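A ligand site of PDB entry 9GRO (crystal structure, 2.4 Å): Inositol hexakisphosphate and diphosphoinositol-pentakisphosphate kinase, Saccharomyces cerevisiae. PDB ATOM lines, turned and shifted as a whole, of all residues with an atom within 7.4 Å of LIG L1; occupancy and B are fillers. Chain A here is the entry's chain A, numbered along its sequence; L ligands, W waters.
The side-chain carboxylate of Glu 43 sits close to the side-chain amide oxygen of Gln 92, 2.8 Å away.
The side-chain carboxylate of Glu 43 is in hydrogen-bond range of the side-chain amide nitrogen of Asn 189, 3.4 Å away.
Water W1 lies within hydrogen-bond range of the side-chain amide nitrogen of Gln 92 (2.7 Å) and the side-chain amino group of Lys 90 (2.9 Å).
N of Asn 189 sits close to N1 of LG2 L2 (3.2 Å).
OE1 of Glu 43 is in salt-bridge range of N4 of LIG L1 (3.6 Å).
The backbone NH of Val 45 sits close to a nitrogen (N2) of LIG L1 (3.5 Å).
A nitrogen (N1) of LG2 L2 sits at hydrogen-bond distance from the side-chain amide oxygen (OD1) of Asn 189 (3.0 Å).
An oxygen (O1) of LG2 L2 sits at hydrogen-bond distance from a nitrogen (N3) of LIG L1, 2.5 Å away.
Merely in contact with LIG L1: Val 44 and Asp 187.
Hydrophobic or aromatic side chains that line LIG L1: Val 44 and Val 45.
Four residues have an atom within 4 Å of LIG L1: Glu 43, Val 44, Val 45 and Asp 187.
Along chain A the residues within 4 Å of LIG L1 span positions 43 to 187.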
ATOM      1  N   HIS A  40     -11.190  35.780  -0.588  1.00  0.00           N
ATOM      2  CA  HIS A  40     -10.208  35.360   0.397  1.00  0.00           C
ATOM      3  C   HIS A  40      -8.995  34.725  -0.285  1.00  0.00           C
ATOM      4  O   HIS A  40      -9.124  34.010  -1.278  1.00  0.00           O
ATOM      5  CB  HIS A  40     -10.819  34.357   1.382  1.00  0.00           C
ATOM      6  CG  HIS A  40     -11.703  34.990   2.414  1.00  0.00           C
ATOM      7  ND1 HIS A  40     -12.932  35.536   2.113  1.00  0.00           N
ATOM      8  CD2 HIS A  40     -11.537  35.159   3.740  1.00  0.00           C
ATOM      9  CE1 HIS A  40     -13.477  36.015   3.216  1.00  0.00           C
ATOM     10  NE2 HIS A  40     -12.651  35.799   4.213  1.00  0.00           N
ATOM     11  N   GLU A  42      -6.742  33.057   1.812  1.00  0.00           N
ATOM     12  CA  GLU A  42      -6.335  32.095   2.824  1.00  0.00           C
ATOM     13  C   GLU A  42      -7.409  31.011   2.893  1.00  0.00           C
ATOM     14  O   GLU A  42      -8.480  31.129   2.298  1.00  0.00           O
ATOM     15  CB  GLU A  42      -6.138  32.759   4.192  1.00  0.00           C
ATOM     16  CG  GLU A  42      -7.028  33.966   4.465  1.00  0.00           C
ATOM     17  CD  GLU A  42      -6.402  34.922   5.481  1.00  0.00           C
ATOM     18  OE1 GLU A  42      -7.112  35.355   6.411  1.00  0.00           O
ATOM     19  OE2 GLU A  42      -5.206  35.238   5.336  1.00  0.00           O
ATOM     20  N   GLU A  43      -7.093  29.932   3.607  1.00  0.00           N
ATOM     21  CA  GLU A  43      -8.027  28.815   3.673  1.00  0.00           C
ATOM     22  C   GLU A  43      -9.385  29.270   4.211  1.00  0.00           C
ATOM     23  O   GLU A  43      -9.469  30.023   5.172  1.00  0.00           O
ATOM     24  CB  GLU A  43      -7.474  27.697   4.557  1.00  0.00           C
ATOM     25  CG  GLU A  43      -8.524  26.666   4.919  1.00  0.00           C
ATOM     26  CD  GLU A  43      -7.937  25.309   5.255  1.00  0.00           C
ATOM     27  OE1 GLU A  43      -6.720  25.251   5.526  1.00  0.00           O
ATOM     28  OE2 GLU A  43      -8.690  24.315   5.233  1.00  0.00           O
ATOM     29  N   VAL A  44     -10.448  28.782   3.570  1.00  0.00           N
ATOM     30  CA  VAL A  44     -11.823  29.118   3.915  1.00  0.00           C
ATOM     31  C   VAL A  44     -12.556  27.826   4.242  1.00  0.00           C
ATOM     32  O   VAL A  44     -12.496  26.858   3.462  1.00  0.00           O
ATOM     33  CB  VAL A  44     -12.522  29.880   2.780  1.00  0.00           C
ATOM     34  CG1 VAL A  44     -13.982  30.160   3.140  1.00  0.00           C
ATOM     35  CG2 VAL A  44     -11.785  31.177   2.465  1.00  0.00           C
ATOM     36  N   VAL A  45     -13.240  27.807   5.378  1.00  0.00           N
ATOM     37  CA  VAL A  45     -14.008  26.648   5.828  1.00  0.00           C
ATOM     38  C   VAL A  45     -15.487  26.990   5.742  1.00  0.00           C
ATOM     39  O   VAL A  45     -15.904  28.066   6.168  1.00  0.00           O
ATOM     40  CB  VAL A  45     -13.628  26.230   7.264  1.00  0.00           C
ATOM     41  CG1 VAL A  45     -14.404  24.997   7.677  1.00  0.00           C
ATOM     42  CG2 VAL A  45     -12.123  25.983   7.363  1.00  0.00           C
ATOM     43  N   ILE A  46     -16.278  26.079   5.181  1.00  0.00           N
ATOM     44  CA  ILE A  46     -17.713  26.251   5.018  1.00  0.00           C
ATOM     45  C   ILE A  46     -18.402  25.149   5.814  1.00  0.00           C
ATOM     46  O   ILE A  46     -18.182  23.962   5.558  1.00  0.00           O
ATOM     47  CB  ILE A  46     -18.129  26.216   3.548  1.00  0.00           C
ATOM     48  CG1 ILE A  46     -17.391  27.315   2.760  1.00  0.00           C
ATOM     49  CG2 ILE A  46     -19.641  26.375   3.410  1.00  0.00           C
ATOM     50  CD1 ILE A  46     -17.527  27.194   1.262  1.00  0.00           C
ATOM     51  N   ARG A  47     -19.258  25.548   6.763  1.00  0.00           N
ATOM     52  CA  ARG A  47     -19.943  24.592   7.631  1.00  0.00           C
ATOM     53  C   ARG A  47     -21.450  24.823   7.621  1.00  0.00           C
ATOM     54  O   ARG A  47     -22.223  23.871   7.759  1.00  0.00           O
ATOM     55  CB  ARG A  47     -19.409  24.692   9.062  1.00  0.00           C
ATOM     56  CG  ARG A  47     -17.996  24.131   9.238  1.00  0.00           C
ATOM     57  CD  ARG A  47     -17.551  24.216  10.691  1.00  0.00           C
ATOM     58  NE  ARG A  47     -16.563  23.189  11.019  1.00  0.00           N
ATOM     59  CZ  ARG A  47     -16.870  21.943  11.370  1.00  0.00           C
ATOM     60  NH1 ARG A  47     -18.124  21.522  11.412  1.00  0.00           N
ATOM     61  NH2 ARG A  47     -15.887  21.099  11.682  1.00  0.00           N
ATOM     62  N   ASP A  51     -24.975  27.587   3.305  1.00  0.00           N
ATOM     63  CA  ASP A  51     -23.832  27.871   2.449  1.00  0.00           C
ATOM     64  C   ASP A  51     -23.417  26.626   1.668  1.00  0.00           C
ATOM     65  O   ASP A  51     -22.988  26.727   0.513  1.00  0.00           O
ATOM     66  CB  ASP A  51     -22.663  28.397   3.272  1.00  0.00           C
ATOM     67  CG  ASP A  51     -22.920  29.797   3.812  1.00  0.00           C
ATOM     68  OD1 ASP A  51     -23.626  30.576   3.144  1.00  0.00           O
ATOM     69  OD2 ASP A  51     -22.402  30.120   4.901  1.00  0.00           O
ATOM     70  N   LYS A  90     -18.210  19.549   6.060  1.00  0.00           N
ATOM     71  CA  LYS A  90     -17.687  20.871   5.794  1.00  0.00           C
ATOM     72  C   LYS A  90     -16.876  20.852   4.508  1.00  0.00           C
ATOM     73  O   LYS A  90     -16.495  19.792   4.006  1.00  0.00           O
ATOM     74  CB  LYS A  90     -16.823  21.396   6.954  1.00  0.00           C
ATOM     75  CG  LYS A  90     -15.560  20.593   7.221  1.00  0.00           C
ATOM     76  CD  LYS A  90     -14.833  21.125   8.451  1.00  0.00           C
ATOM     77  CE  LYS A  90     -13.558  20.368   8.750  1.00  0.00           C
ATOM     78  NZ  LYS A  90     -12.885  20.898   9.960  1.00  0.00           N
ATOM     79  N   GLN A  92     -13.447  22.790   2.705  1.00  0.00           N
ATOM     80  CA  GLN A  92     -12.267  23.613   2.874  1.00  0.00           C
ATOM     81  C   GLN A  92     -11.743  24.030   1.509  1.00  0.00           C
ATOM     82  O   GLN A  92     -11.572  23.179   0.627  1.00  0.00           O
ATOM     83  CB  GLN A  92     -11.191  22.861   3.666  1.00  0.00           C
ATOM     84  CG  GLN A  92     -11.567  22.579   5.105  1.00  0.00           C
ATOM     85  CD  GLN A  92     -10.457  21.931   5.903  1.00  0.00           C
ATOM     86  OE1 GLN A  92      -9.386  21.630   5.365  1.00  0.00           O
ATOM     87  NE2 GLN A  92     -10.694  21.720   7.195  1.00  0.00           N
ATOM     88  N   LYS A  94      -8.566  25.760  -0.143  1.00  0.00           N
ATOM     89  CA  LYS A  94      -7.195  26.202   0.058  1.00  0.00           C
ATOM     90  C   LYS A  94      -6.698  26.887  -1.208  1.00  0.00           C
ATOM     91  O   LYS A  94      -6.419  26.197  -2.194  1.00  0.00           O
ATOM     92  CB  LYS A  94      -6.296  25.021   0.423  1.00  0.00           C
ATOM     93  CG  LYS A  94      -6.408  24.571   1.877  1.00  0.00           C
ATOM     94  CD  LYS A  94      -6.707  23.078   1.994  1.00  0.00           C
ATOM     95  CE  LYS A  94      -5.512  22.291   2.490  1.00  0.00           C
ATOM     96  NZ  LYS A  94      -5.919  20.924   2.923  1.00  0.00           N
ATOM     97  N   LYS A 111     -15.165  17.254   3.374  1.00  0.00           N
ATOM     98  CA  LYS A 111     -14.969  16.369   4.508  1.00  0.00           C
ATOM     99  C   LYS A 111     -16.315  16.055   5.155  1.00  0.00           C
ATOM    100  O   LYS A 111     -17.209  16.906   5.192  1.00  0.00           O
ATOM    101  CB  LYS A 111     -14.040  16.987   5.554  1.00  0.00           C
ATOM    102  CG  LYS A 111     -12.566  16.757   5.288  1.00  0.00           C
ATOM    103  CD  LYS A 111     -11.720  17.893   5.841  1.00  0.00           C
ATOM    104  CE  LYS A 111     -10.394  17.391   6.365  1.00  0.00           C
ATOM    105  NZ  LYS A 111      -9.347  18.441   6.306  1.00  0.00           N
ATOM    106  N   LYS A 182      -9.041  27.707  19.554  1.00  0.00           N
ATOM    107  CA  LYS A 182      -8.745  27.265  18.196  1.00  0.00           C
ATOM    108  C   LYS A 182      -7.258  27.412  17.893  1.00  0.00           C
ATOM    109  O   LYS A 182      -6.666  26.558  17.222  1.00  0.00           O
ATOM    110  CB  LYS A 182      -9.567  28.069  17.191  1.00  0.00           C
ATOM    111  CG  LYS A 182     -11.026  27.630  17.037  1.00  0.00           C
ATOM    112  CD  LYS A 182     -11.936  28.730  16.468  1.00  0.00           C
ATOM    113  CE  LYS A 182     -11.217  29.725  15.563  1.00  0.00           C
ATOM    114  NZ  LYS A 182     -11.974  31.008  15.492  1.00  0.00           N
ATOM    115  N   ASP A 186      -6.922  23.374  17.531  1.00  0.00           N
ATOM    116  CA  ASP A 186      -7.381  23.006  16.195  1.00  0.00           C
ATOM    117  C   ASP A 186      -6.178  22.764  15.289  1.00  0.00           C
ATOM    118  O   ASP A 186      -5.039  23.115  15.605  1.00  0.00           O
ATOM    119  CB  ASP A 186      -8.280  24.088  15.614  1.00  0.00           C
ATOM    120  CG  ASP A 186      -9.620  24.176  16.321  1.00  0.00           C
ATOM    121  OD1 ASP A 186      -9.792  23.518  17.361  1.00  0.00           O
ATOM    122  OD2 ASP A 186     -10.493  24.914  15.822  1.00  0.00           O
ATOM    123  N   ASP A 187      -6.435  22.142  14.136  1.00  0.00           N
ATOM    124  CA  ASP A 187      -5.387  21.960  13.151  1.00  0.00           C
ATOM    125  C   ASP A 187      -4.929  23.323  12.612  1.00  0.00           C
ATOM    126  O   ASP A 187      -5.707  24.263  12.502  1.00  0.00           O
ATOM    127  CB  ASP A 187      -5.868  21.098  11.983  1.00  0.00           C
ATOM    128  CG  ASP A 187      -5.974  19.639  12.360  1.00  0.00           C
ATOM    129  OD1 ASP A 187      -5.416  19.240  13.396  1.00  0.00           O
ATOM    130  OD2 ASP A 187      -6.632  18.886  11.606  1.00  0.00           O
ATOM    131  N   SER A 188      -3.646  23.395  12.269  1.00  0.00           N
ATOM    132  CA  SER A 188      -3.068  24.587  11.666  1.00  0.00           C
ATOM    133  C   SER A 188      -2.436  24.192  10.347  1.00  0.00           C
ATOM    134  O   SER A 188      -1.669  23.218  10.273  1.00  0.00           O
ATOM    135  CB  SER A 188      -2.022  25.218  12.591  1.00  0.00           C
ATOM    136  OG  SER A 188      -0.936  24.340  12.800  1.00  0.00           O
ATOM    137  N   ASN A 189      -2.750  24.935   9.287  1.00  0.00           N
ATOM    138  CA  ASN A 189      -2.145  24.728   7.989  1.00  0.00           C
ATOM    139  C   ASN A 189      -0.744  25.327   7.895  1.00  0.00           C
ATOM    140  O   ASN A 189      -0.211  25.461   6.786  1.00  0.00           O
ATOM    141  CB  ASN A 189      -3.031  25.310   6.888  1.00  0.00           C
ATOM    142  CG  ASN A 189      -3.207  26.815   7.008  1.00  0.00           C
ATOM    143  OD1 ASN A 189      -2.500  27.471   7.772  1.00  0.00           O
ATOM    144  ND2 ASN A 189      -4.142  27.362   6.243  1.00  0.00           N
ATOM    145  N   ALA A 190      -0.145  25.702   9.030  1.00  0.00           N
ATOM    146  CA  ALA A 190       1.199  26.265   9.022  1.00  0.00           C
ATOM    147  C   ALA A 190       2.224  25.263   8.492  1.00  0.00           C
ATOM    148  O   ALA A 190       3.130  25.623   7.743  1.00  0.00           O
ATOM    149  CB  ALA A 190       1.579  26.727  10.424  1.00  0.00           C
HETATM  150  N1  LIG L   1     -15.956  31.625   6.239  1.00  0.00           N
HETATM  151  C1  LIG L   1     -15.653  30.888   7.464  1.00  0.00           C
HETATM  152  C2  LIG L   1     -14.714  31.718   8.336  1.00  0.00           C
HETATM  153  C3  LIG L   1     -13.408  32.029   7.598  1.00  0.00           C
HETATM  154  N2  LIG L   1     -12.788  30.819   7.078  1.00  0.00           N
HETATM  155  C4  LIG L   1     -11.833  30.238   8.016  1.00  0.00           C
HETATM  156  C5  LIG L   1     -10.531  31.050   8.081  1.00  0.00           C
HETATM  157  C6  LIG L   1      -9.644  30.612   9.263  1.00  0.00           C
HETATM  158  C7  LIG L   1      -9.750  29.103   9.474  1.00  0.00           C
HETATM  159  N3  LIG L   1      -8.502  28.522   9.947  1.00  0.00           N
HETATM  160  C8  LIG L   1      -7.861  27.765   8.879  1.00  0.00           C
HETATM  161  C9  LIG L   1      -8.647  26.517   8.470  1.00  0.00           C
HETATM  162  C10 LIG L   1      -8.374  25.344   9.406  1.00  0.00           C
HETATM  163  N4  LIG L   1      -7.091  24.770   9.039  1.00  0.00           N
HETATM  164  N1  LG2 L   2      -4.204  27.644  10.221  1.00  0.00           N
HETATM  165  C1  LG2 L   2      -4.156  28.374  11.398  1.00  0.00           C
HETATM  166  C2  LG2 L   2      -3.200  29.546  11.202  1.00  0.00           C
HETATM  167  C3  LG2 L   2      -1.732  29.171  11.062  1.00  0.00           C
HETATM  168  C4  LG2 L   2      -1.094  29.681   9.777  1.00  0.00           C
HETATM  169  N2  LG2 L   2      -1.268  31.024   9.627  1.00  0.00           N
HETATM  170  C5  LG2 L   2      -5.523  28.863  11.827  1.00  0.00           C
HETATM  171  O1  LG2 L   2      -6.326  29.285  10.988  1.00  0.00           O
HETATM  172  O2  LG2 L   2      -5.732  28.795  13.059  1.00  0.00           O
HETATM  173  O   HOH W   1     -11.047  23.120   9.436  1.00  0.00           O
